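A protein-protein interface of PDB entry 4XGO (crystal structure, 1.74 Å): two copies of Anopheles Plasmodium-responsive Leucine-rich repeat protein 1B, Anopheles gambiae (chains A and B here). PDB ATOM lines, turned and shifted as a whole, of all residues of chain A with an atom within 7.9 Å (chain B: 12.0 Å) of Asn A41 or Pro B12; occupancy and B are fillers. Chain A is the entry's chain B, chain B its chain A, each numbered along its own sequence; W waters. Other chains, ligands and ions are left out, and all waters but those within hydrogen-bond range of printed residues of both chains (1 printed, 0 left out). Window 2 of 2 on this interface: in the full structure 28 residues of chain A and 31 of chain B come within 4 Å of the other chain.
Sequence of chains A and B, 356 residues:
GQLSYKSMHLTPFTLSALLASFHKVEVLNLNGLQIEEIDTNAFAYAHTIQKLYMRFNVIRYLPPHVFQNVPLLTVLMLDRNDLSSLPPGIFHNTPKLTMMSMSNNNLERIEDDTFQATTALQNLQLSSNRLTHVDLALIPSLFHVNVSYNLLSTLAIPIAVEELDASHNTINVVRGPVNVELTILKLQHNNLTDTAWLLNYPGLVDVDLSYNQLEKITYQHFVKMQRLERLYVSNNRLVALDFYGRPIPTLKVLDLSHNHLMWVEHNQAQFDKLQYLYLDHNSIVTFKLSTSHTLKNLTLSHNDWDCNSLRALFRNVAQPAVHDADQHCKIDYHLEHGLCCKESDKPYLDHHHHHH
The backbone carbonyl oxygen (O) of Leu B10 lies within hydrogen-bond range of the backbone NH (N) of Asp A39 (2.9 Å). N of Leu B10 is in hydrogen-bond range of O of Glu A37, at 2.8 Å. The side-chain carboxylate of Glu A37 sits at hydrogen-bond distance from a ring nitrogen (ND1) of His B9 (3.3 Å).
The backbone carbonyl oxygen of His B9 lies within hydrogen-bond range of the side-chain hydroxyl of Thr B14 (2.8 Å). The side-chain hydroxyl (OG1) of Thr B11 lies close to the backbone NH (N) of Phe B13 (3.3 Å). The side-chain hydroxyl (OG1) of Thr B14 sits at hydrogen-bond distance from the backbone NH (N) of Thr B11, at 2.8 Å. The side-chain carboxylate (OE2) of Glu A37 sits at hydrogen-bond distance from the backbone NH (N) of Asp A39 (3.3 Å).
Among the printed residues, merely in contact across the chains: Asp A39 with Thr B11, Ala A42 with Leu B15, Asn A41 with Pro B12, Ile A38 with Leu B10, Glu A37 with Met B8, Ala A42 with Leu B10, Phe A43 with Leu B10, Asp A39 with Pro B12 and Phe A43 with Leu B15.
Of the printed residues of chain B, Ile A38 touches Leu B10 (3.6 Å). Of the printed residues of chain B, Asn A41 touches Pro B12. Of chain B, only Leu B10 and Leu B15 come within 4 Å of Ala A42. Phe A43 touches just these residues of chain B: Leu B10 (3.7 Å) and Leu B15 (3.9 Å). No residue of chain B comes within 4 Å of Ala A44. Printed residues of chain A within 4 Å of Met B8: Glu A37 (3.7 Å). Of the printed residues of chain A, His B9 touches Glu A37 (3.3 Å). Of the printed residues of chain A, Leu B10 touches Glu A37 (2.8 Å), Ile A38 (3.6 Å), Asp A39 (2.9 Å), Ala A42 (3.7 Å) and Phe A43 (3.7 Å). Printed residues of chain A within 4 Å of Thr B11: Asp A39. Pro B12 touches two residues of chain A. Ser B16 touches none of the printed residues of chain A. The nearest residue of chain A that does not touch Pro B12 is Ala A42 (4.3 Å). The nearest printed residue of chain A that does not touch His B9 is Asp A39 (5.1 Å).
Printed residues of chain B that touch a printed residue of chain A: Met B8, His B9, Leu B10, Thr B11, Pro B12 and Leu B15. Hydrophobic or aromatic side chains of chain B that line the printed part of chain A: His B9, Leu B10, Pro B12 and Leu B15. Hydrophobic or aromatic side chains of chain A within 4 Å of the printed part of chain B: Ala A42 and Phe A43.
No position is printed for both chains.
Water W1 lies within hydrogen-bond range of a ring nitrogen (ND1) of His B9 (2.7 Å), the side-chain carboxylate (OD1) of Asp A39 (2.9 Å) and the side-chain carboxylate (OE1) of Glu A37 (3.1 Å).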
ATOM      1  N   GLU A  37      29.531 -11.060 -31.357  1.00  0.00           N
ATOM      2  CA  GLU A  37      29.883 -12.464 -31.428  1.00  0.00           C
ATOM      3  C   GLU A  37      28.651 -13.219 -30.985  1.00  0.00           C
ATOM      4  O   GLU A  37      27.914 -12.742 -30.119  1.00  0.00           O
ATOM      5  CB  GLU A  37      31.045 -12.771 -30.490  1.00  0.00           C
ATOM      6  CG  GLU A  37      31.479 -14.230 -30.488  1.00  0.00           C
ATOM      7  CD  GLU A  37      30.659 -15.140 -29.588  1.00  0.00           C
ATOM      8  OE1 GLU A  37      29.877 -14.651 -28.746  1.00  0.00           O
ATOM      9  OE2 GLU A  37      30.831 -16.379 -29.730  1.00  0.00           O
ATOM     10  N   ILE A  38      28.434 -14.382 -31.608  1.00  0.00           N
ATOM     11  CA  ILE A  38      27.356 -15.290 -31.244  1.00  0.00           C
ATOM     12  C   ILE A  38      27.931 -16.694 -31.047  1.00  0.00           C
ATOM     13  O   ILE A  38      28.637 -17.184 -31.922  1.00  0.00           O
ATOM     14  CB  ILE A  38      26.284 -15.331 -32.354  1.00  0.00           C
ATOM     15  CG1 ILE A  38      25.722 -13.918 -32.586  1.00  0.00           C
ATOM     16  CG2 ILE A  38      25.164 -16.288 -31.983  1.00  0.00           C
ATOM     17  CD1 ILE A  38      24.798 -13.839 -33.784  1.00  0.00           C
ATOM     18  N   ASP A  39      27.675 -17.304 -29.885  1.00  0.00           N
ATOM     19  CA  ASP A  39      28.076 -18.702 -29.635  1.00  0.00           C
ATOM     20  C   ASP A  39      27.245 -19.663 -30.498  1.00  0.00           C
ATOM     21  O   ASP A  39      26.064 -19.423 -30.730  1.00  0.00           O
ATOM     22  CB  ASP A  39      27.883 -19.082 -28.158  1.00  0.00           C
ATOM     23  CG  ASP A  39      28.924 -18.470 -27.220  1.00  0.00           C
ATOM     24  OD1 ASP A  39      29.808 -17.709 -27.655  1.00  0.00           O
ATOM     25  OD2 ASP A  39      28.845 -18.760 -26.004  1.00  0.00           O
ATOM     26  N   THR A  40      27.853 -20.772 -30.935  1.00  0.00           N
ATOM     27  CA  THR A  40      27.138 -21.822 -31.690  1.00  0.00           C
ATOM     28  C   THR A  40      25.816 -22.226 -31.055  1.00  0.00           C
ATOM     29  O   THR A  40      24.821 -22.422 -31.755  1.00  0.00           O
ATOM     30  CB  THR A  40      28.019 -23.082 -31.870  1.00  0.00           C
ATOM     31  OG1 THR A  40      29.028 -22.784 -32.828  1.00  0.00           O
ATOM     32  CG2 THR A  40      27.213 -24.298 -32.360  1.00  0.00           C
ATOM     33  N   ASN A  41      25.802 -22.323 -29.730  1.00  0.00           N
ATOM     34  CA  ASN A  41      24.618 -22.802 -29.034  1.00  0.00           C
ATOM     35  C   ASN A  41      23.764 -21.707 -28.425  1.00  0.00           C
ATOM     36  O   ASN A  41      22.924 -21.989 -27.576  1.00  0.00           O
ATOM     37  CB  ASN A  41      24.986 -23.845 -27.968  1.00  0.00           C
ATOM     38  CG  ASN A  41      25.839 -23.281 -26.853  1.00  0.00           C
ATOM     39  OD1 ASN A  41      26.319 -22.162 -26.925  1.00  0.00           O
ATOM     40  ND2 ASN A  41      26.075 -24.096 -25.824  1.00  0.00           N
ATOM     41  N   ALA A  42      23.960 -20.463 -28.864  1.00  0.00           N
ATOM     42  CA  ALA A  42      23.136 -19.357 -28.364  1.00  0.00           C
ATOM     43  C   ALA A  42      21.638 -19.635 -28.465  1.00  0.00           C
ATOM     44  O   ALA A  42      20.890 -19.317 -27.532  1.00  0.00           O
ATOM     45  CB  ALA A  42      23.478 -18.073 -29.100  1.00  0.00           C
ATOM     46  N   PHE A  43      21.195 -20.224 -29.572  1.00  0.00           N
ATOM     47  CA  PHE A  43      19.771 -20.504 -29.789  1.00  0.00           C
ATOM     48  C   PHE A  43      19.446 -21.987 -29.614  1.00  0.00           C
ATOM     49  O   PHE A  43      18.495 -22.496 -30.214  1.00  0.00           O
ATOM     50  CB  PHE A  43      19.328 -20.032 -31.183  1.00  0.00           C
ATOM     51  CG  PHE A  43      19.568 -18.565 -31.415  1.00  0.00           C
ATOM     52  CD1 PHE A  43      18.837 -17.609 -30.715  1.00  0.00           C
ATOM     53  CD2 PHE A  43      20.523 -18.136 -32.326  1.00  0.00           C
ATOM     54  CE1 PHE A  43      19.071 -16.268 -30.918  1.00  0.00           C
ATOM     55  CE2 PHE A  43      20.761 -16.788 -32.527  1.00  0.00           C
ATOM     56  CZ  PHE A  43      20.033 -15.854 -31.822  1.00  0.00           C
ATOM     57  N   ALA A  44      20.224 -22.674 -28.789  1.00  0.00           N
ATOM     58  CA  ALA A  44      20.043 -24.117 -28.635  1.00  0.00           C
ATOM     59  C   ALA A  44      18.707 -24.495 -28.024  1.00  0.00           C
ATOM     60  O   ALA A  44      18.179 -25.573 -28.326  1.00  0.00           O
ATOM     61  CB  ALA A  44      21.189 -24.715 -27.837  1.00  0.00           C
ATOM     62  N   TYR A  45      18.161 -23.627 -27.174  1.00  0.00           N
ATOM     63  CA  TYR A  45      16.905 -23.911 -26.463  1.00  0.00           C
ATOM     64  C   TYR A  45      15.826 -22.902 -26.816  1.00  0.00           C
ATOM     65  O   TYR A  45      14.990 -22.551 -25.971  1.00  0.00           O
ATOM     66  CB  TYR A  45      17.151 -23.934 -24.944  1.00  0.00           C
ATOM     67  CG  TYR A  45      18.140 -25.005 -24.537  1.00  0.00           C
ATOM     68  CD1 TYR A  45      17.842 -26.358 -24.702  1.00  0.00           C
ATOM     69  CD2 TYR A  45      19.377 -24.666 -24.009  1.00  0.00           C
ATOM     70  CE1 TYR A  45      18.751 -27.338 -24.346  1.00  0.00           C
ATOM     71  CE2 TYR A  45      20.293 -25.633 -23.651  1.00  0.00           C
ATOM     72  CZ  TYR A  45      19.984 -26.963 -23.820  1.00  0.00           C
ATOM     73  OH  TYR A  45      20.917 -27.912 -23.465  1.00  0.00           O
ATOM     74  N   ALA A  46      15.829 -22.438 -28.064  1.00  0.00           N
ATOM     75  CA  ALA A  46      14.873 -21.426 -28.505  1.00  0.00           C
ATOM     76  C   ALA A  46      14.029 -21.937 -29.666  1.00  0.00           C
ATOM     77  O   ALA A  46      13.763 -21.218 -30.626  1.00  0.00           O
ATOM     78  CB  ALA A  46      15.596 -20.135 -28.865  1.00  0.00           C
ATOM     79  N   PRO A  63      28.255 -18.491 -36.391  1.00  0.00           N
ATOM     80  CA  PRO A  63      28.973 -19.737 -36.127  1.00  0.00           C
ATOM     81  C   PRO A  63      28.299 -20.958 -36.737  1.00  0.00           C
ATOM     82  O   PRO A  63      27.110 -20.912 -37.075  1.00  0.00           O
ATOM     83  CB  PRO A  63      28.940 -19.821 -34.604  1.00  0.00           C
ATOM     84  CG  PRO A  63      27.665 -19.186 -34.231  1.00  0.00           C
ATOM     85  CD  PRO A  63      27.483 -18.046 -35.217  1.00  0.00           C
ATOM     86  N   PRO A  64      29.049 -22.062 -36.883  1.00  0.00           N
ATOM     87  CA  PRO A  64      28.433 -23.262 -37.396  1.00  0.00           C
ATOM     88  C   PRO A  64      27.210 -23.657 -36.590  1.00  0.00           C
ATOM     89  O   PRO A  64      27.173 -23.426 -35.388  1.00  0.00           O
ATOM     90  CB  PRO A  64      29.521 -24.335 -37.227  1.00  0.00           C
ATOM     91  CG  PRO A  64      30.803 -23.587 -37.145  1.00  0.00           C
ATOM     92  CD  PRO A  64      30.493 -22.236 -36.611  1.00  0.00           C
ATOM     93  N   HIS A  65      26.208 -24.174 -37.286  1.00  0.00           N
ATOM     94  CA  HIS A  65      25.001 -24.696 -36.654  1.00  0.00           C
ATOM     95  C   HIS A  65      24.186 -23.638 -35.891  1.00  0.00           C
ATOM     96  O   HIS A  65      23.321 -23.977 -35.075  1.00  0.00           O
ATOM     97  CB  HIS A  65      25.354 -25.875 -35.736  1.00  0.00           C
ATOM     98  CG  HIS A  65      25.853 -27.085 -36.467  1.00  0.00           C
ATOM     99  ND1 HIS A  65      26.630 -28.051 -35.866  1.00  0.00           N
ATOM    100  CD2 HIS A  65      25.689 -27.480 -37.753  1.00  0.00           C
ATOM    101  CE1 HIS A  65      26.921 -28.990 -36.748  1.00  0.00           C
ATOM    102  NE2 HIS A  65      26.366 -28.666 -37.902  1.00  0.00           N
ATOM    103  N   VAL A  66      24.406 -22.354 -36.165  1.00  0.00           N
ATOM    104  CA  VAL A  66      23.742 -21.317 -35.380  1.00  0.00           C
ATOM    105  C   VAL A  66      22.202 -21.460 -35.379  1.00  0.00           C
ATOM    106  O   VAL A  66      21.554 -21.199 -34.352  1.00  0.00           O
ATOM    107  CB  VAL A  66      24.160 -19.896 -35.834  1.00  0.00           C
ATOM    108  CG1 VAL A  66      23.692 -19.638 -37.253  1.00  0.00           C
ATOM    109  CG2 VAL A  66      23.633 -18.838 -34.867  1.00  0.00           C
ATOM    110  N   GLN A  68      20.507 -24.333 -36.102  1.00  0.00           N
ATOM    111  CA  GLN A  68      20.158 -25.741 -36.104  1.00  0.00           C
ATOM    112  C   GLN A  68      18.913 -26.035 -35.260  1.00  0.00           C
ATOM    113  O   GLN A  68      18.188 -26.985 -35.555  1.00  0.00           O
ATOM    114  CB  GLN A  68      21.343 -26.560 -35.605  1.00  0.00           C
ATOM    115  CG  GLN A  68      21.189 -28.060 -35.716  1.00  0.00           C
ATOM    116  CD  GLN A  68      22.508 -28.758 -35.463  1.00  0.00           C
ATOM    117  OE1 GLN A  68      22.955 -29.587 -36.259  1.00  0.00           O
ATOM    118  NE2 GLN A  68      23.156 -28.410 -34.352  1.00  0.00           N
ATOM    119  N   ASN A  69      18.664 -25.252 -34.218  1.00  0.00           N
ATOM    120  CA  ASN A  69      17.524 -25.528 -33.325  1.00  0.00           C
ATOM    121  C   ASN A  69      16.403 -24.504 -33.405  1.00  0.00           C
ATOM    122  O   ASN A  69      15.724 -24.265 -32.410  1.00  0.00           O
ATOM    123  CB  ASN A  69      17.995 -25.612 -31.874  1.00  0.00           C
ATOM    124  CG  ASN A  69      18.959 -26.735 -31.646  1.00  0.00           C
ATOM    125  OD1 ASN A  69      20.069 -26.518 -31.163  1.00  0.00           O
ATOM    126  ND2 ASN A  69      18.554 -27.948 -31.999  1.00  0.00           N
ATOM    127  N   MET B   8      28.643  -6.721 -27.192  1.00  0.00           N
ATOM    128  CA  MET B   8      28.311  -7.879 -26.360  1.00  0.00           C
ATOM    129  C   MET B   8      28.477  -9.178 -27.128  1.00  0.00           C
ATOM    130  O   MET B   8      28.416  -9.205 -28.364  1.00  0.00           O
ATOM    131  CB  MET B   8      26.890  -7.764 -25.809  1.00  0.00           C
ATOM    132  CG  MET B   8      25.755  -8.003 -26.800  1.00  0.00           C
ATOM    133  SD  MET B   8      24.116  -8.097 -26.023  1.00  0.00           S
ATOM    134  CE  MET B   8      24.044  -9.821 -25.619  1.00  0.00           C
ATOM    135  N   HIS B   9      28.736 -10.250 -26.377  1.00  0.00           N
ATOM    136  CA  HIS B   9      28.747 -11.610 -26.910  1.00  0.00           C
ATOM    137  C   HIS B   9      27.378 -12.212 -26.599  1.00  0.00           C
ATOM    138  O   HIS B   9      26.895 -12.107 -25.455  1.00  0.00           O
ATOM    139  CB  HIS B   9      29.844 -12.466 -26.231  1.00  0.00           C
ATOM    140  CG  HIS B   9      31.232 -12.219 -26.748  1.00  0.00           C
ATOM    141  ND1 HIS B   9      32.154 -13.236 -26.896  1.00  0.00           N
ATOM    142  CD2 HIS B   9      31.857 -11.086 -27.151  1.00  0.00           C
ATOM    143  CE1 HIS B   9      33.284 -12.738 -27.370  1.00  0.00           C
ATOM    144  NE2 HIS B   9      33.131 -11.434 -27.527  1.00  0.00           N
ATOM    145  N   LEU B  10      26.733 -12.811 -27.591  1.00  0.00           N
ATOM    146  CA  LEU B  10      25.482 -13.499 -27.381  1.00  0.00           C
ATOM    147  C   LEU B  10      25.755 -14.966 -27.059  1.00  0.00           C
ATOM    148  O   LEU B  10      26.112 -15.756 -27.937  1.00  0.00           O
ATOM    149  CB  LEU B  10      24.565 -13.396 -28.589  1.00  0.00           C
ATOM    150  CG  LEU B  10      23.116 -13.805 -28.299  1.00  0.00           C
ATOM    151  CD1 LEU B  10      22.452 -12.792 -27.390  1.00  0.00           C
ATOM    152  CD2 LEU B  10      22.333 -13.954 -29.597  1.00  0.00           C
ATOM    153  N   THR B  11      25.569 -15.307 -25.788  1.00  0.00           N
ATOM    154  CA  THR B  11      25.853 -16.650 -25.268  1.00  0.00           C
ATOM    155  C   THR B  11      24.578 -17.176 -24.623  1.00  0.00           C
ATOM    156  O   THR B  11      23.623 -16.418 -24.420  1.00  0.00           O
ATOM    157  CB  THR B  11      27.033 -16.607 -24.263  1.00  0.00           C
ATOM    158  OG1 THR B  11      26.615 -16.078 -22.989  1.00  0.00           O
ATOM    159  CG2 THR B  11      28.164 -15.766 -24.800  1.00  0.00           C
ATOM    160  N   PRO B  12      24.505 -18.487 -24.322  1.00  0.00           N
ATOM    161  CA  PRO B  12      23.325 -18.885 -23.587  1.00  0.00           C
ATOM    162  C   PRO B  12      23.085 -18.077 -22.305  1.00  0.00           C
ATOM    163  O   PRO B  12      21.948 -17.810 -21.991  1.00  0.00           O
ATOM    164  CB  PRO B  12      23.584 -20.372 -23.291  1.00  0.00           C
ATOM    165  CG  PRO B  12      24.423 -20.802 -24.448  1.00  0.00           C
ATOM    166  CD  PRO B  12      25.338 -19.653 -24.686  1.00  0.00           C
ATOM    167  N   PHE B  13      24.143 -17.678 -21.607  1.00  0.00           N
ATOM    168  CA  PHE B  13      24.020 -16.852 -20.413  1.00  0.00           C
ATOM    169  C   PHE B  13      23.459 -15.463 -20.765  1.00  0.00           C
ATOM    170  O   PHE B  13      22.448 -15.043 -20.207  1.00  0.00           O
ATOM    171  CB  PHE B  13      25.355 -16.710 -19.685  1.00  0.00           C
ATOM    172  CG  PHE B  13      25.286 -15.859 -18.440  1.00  0.00           C
ATOM    173  CD1 PHE B  13      24.906 -16.431 -17.222  1.00  0.00           C
ATOM    174  CD2 PHE B  13      25.589 -14.489 -18.476  1.00  0.00           C
ATOM    175  CE1 PHE B  13      24.832 -15.665 -16.069  1.00  0.00           C
ATOM    176  CE2 PHE B  13      25.511 -13.723 -17.318  1.00  0.00           C
ATOM    177  CZ  PHE B  13      25.125 -14.324 -16.114  1.00  0.00           C
ATOM    178  N   THR B  14      24.079 -14.767 -21.709  1.00  0.00           N
ATOM    179  CA  THR B  14      23.631 -13.413 -21.979  1.00  0.00           C
ATOM    180  C   THR B  14      22.228 -13.410 -22.596  1.00  0.00           C
ATOM    181  O   THR B  14      21.422 -12.498 -22.313  1.00  0.00           O
ATOM    182  CB  THR B  14      24.620 -12.615 -22.843  1.00  0.00           C
ATOM    183  OG1 THR B  14      24.785 -13.255 -24.114  1.00  0.00           O
ATOM    184  CG2 THR B  14      25.973 -12.513 -22.148  1.00  0.00           C
ATOM    185  N   LEU B  15      21.910 -14.412 -23.418  1.00  0.00           N
ATOM    186  CA  LEU B  15      20.561 -14.497 -23.962  1.00  0.00           C
ATOM    187  C   LEU B  15      19.543 -14.812 -22.854  1.00  0.00           C
ATOM    188  O   LEU B  15      18.444 -14.251 -22.837  1.00  0.00           O
ATOM    189  CB  LEU B  15      20.469 -15.484 -25.128  1.00  0.00           C
ATOM    190  CG  LEU B  15      19.068 -15.626 -25.753  1.00  0.00           C
ATOM    191  CD1 LEU B  15      18.505 -14.292 -26.222  1.00  0.00           C
ATOM    192  CD2 LEU B  15      19.034 -16.638 -26.892  1.00  0.00           C
ATOM    193  N   SER B  16      19.921 -15.682 -21.909  1.00  0.00           N
ATOM    194  CA  SER B  16      19.048 -15.994 -20.769  1.00  0.00           C
ATOM    195  C   SER B  16      18.738 -14.732 -19.971  1.00  0.00           C
ATOM    196  O   SER B  16      17.570 -14.482 -19.614  1.00  0.00           O
ATOM    197  CB  SER B  16      19.690 -17.044 -19.851  1.00  0.00           C
ATOM    198  OG  SER B  16      18.805 -17.427 -18.807  1.00  0.00           O
ATOM    199  N   ALA B  17      19.769 -13.947 -19.692  1.00  0.00           N
ATOM    200  CA  ALA B  17      19.594 -12.721 -18.915  1.00  0.00           C
ATOM    201  C   ALA B  17      18.714 -11.718 -19.658  1.00  0.00           C
ATOM    202  O   ALA B  17      17.815 -11.113 -19.061  1.00  0.00           O
ATOM    203  CB  ALA B  17      20.930 -12.133 -18.517  1.00  0.00           C
ATOM    204  N   LEU B  18      18.948 -11.560 -20.957  1.00  0.00           N
ATOM    205  CA  LEU B  18      18.077 -10.742 -21.799  1.00  0.00           C
ATOM    206  C   LEU B  18      16.622 -11.185 -21.790  1.00  0.00           C
ATOM    207  O   LEU B  18      15.726 -10.377 -21.601  1.00  0.00           O
ATOM    208  CB  LEU B  18      18.561 -10.749 -23.249  1.00  0.00           C
ATOM    209  CG  LEU B  18      19.669  -9.801 -23.641  1.00  0.00           C
ATOM    210  CD1 LEU B  18      20.084 -10.133 -25.069  1.00  0.00           C
ATOM    211  CD2 LEU B  18      19.225  -8.348 -23.514  1.00  0.00           C
ATOM    212  N   LEU B  19      16.389 -12.471 -22.034  1.00  0.00           N
ATOM    213  CA  LEU B  19      15.025 -13.019 -22.046  1.00  0.00           C
ATOM    214  C   LEU B  19      14.318 -12.804 -20.704  1.00  0.00           C
ATOM    215  O   LEU B  19      13.140 -12.473 -20.683  1.00  0.00           O
ATOM    216  CB  LEU B  19      15.028 -14.517 -22.408  1.00  0.00           C
ATOM    217  CG  LEU B  19      15.471 -14.854 -23.841  1.00  0.00           C
ATOM    218  CD1 LEU B  19      15.724 -16.348 -24.016  1.00  0.00           C
ATOM    219  CD2 LEU B  19      14.492 -14.336 -24.891  1.00  0.00           C
ATOM    220  N   ALA B  20      15.049 -12.947 -19.597  1.00  0.00           N
ATOM    221  CA  ALA B  20      14.474 -12.731 -18.259  1.00  0.00           C
ATOM    222  C   ALA B  20      14.039 -11.275 -18.093  1.00  0.00           C
ATOM    223  O   ALA B  20      12.957 -10.988 -17.555  1.00  0.00           O
ATOM    224  CB  ALA B  20      15.477 -13.096 -17.180  1.00  0.00           C
ATOM    225  N   SER B  21      14.887 -10.350 -18.557  1.00  0.00           N
ATOM    226  CA  SER B  21      14.556  -8.917 -18.490  1.00  0.00           C
ATOM    227  C   SER B  21      13.339  -8.572 -19.378  1.00  0.00           C
ATOM    228  O   SER B  21      12.515  -7.728 -19.023  1.00  0.00           O
ATOM    229  CB  SER B  21      15.809  -8.079 -18.837  1.00  0.00           C
ATOM    230  OG  SER B  21      16.083  -8.051 -20.233  1.00  0.00           O
ATOM    231  N   PHE B  22      13.225  -9.233 -20.527  1.00  0.00           N
ATOM    232  CA  PHE B  22      12.125  -9.022 -21.450  1.00  0.00           C
ATOM    233  C   PHE B  22      10.839  -9.586 -20.849  1.00  0.00           C
ATOM    234  O   PHE B  22       9.788  -8.957 -20.930  1.00  0.00           O
ATOM    235  CB  PHE B  22      12.344  -9.738 -22.780  1.00  0.00           C
ATOM    236  CG  PHE B  22      13.482  -9.202 -23.613  1.00  0.00           C
ATOM    237  CD1 PHE B  22      14.097  -7.979 -23.329  1.00  0.00           C
ATOM    238  CD2 PHE B  22      13.913  -9.922 -24.722  1.00  0.00           C
ATOM    239  CE1 PHE B  22      15.117  -7.507 -24.130  1.00  0.00           C
ATOM    240  CE2 PHE B  22      14.934  -9.447 -25.520  1.00  0.00           C
ATOM    241  CZ  PHE B  22      15.533  -8.241 -25.225  1.00  0.00           C
HETATM  242  O   HOH W   1      31.366 -15.698 -26.206  1.00  0.00           O
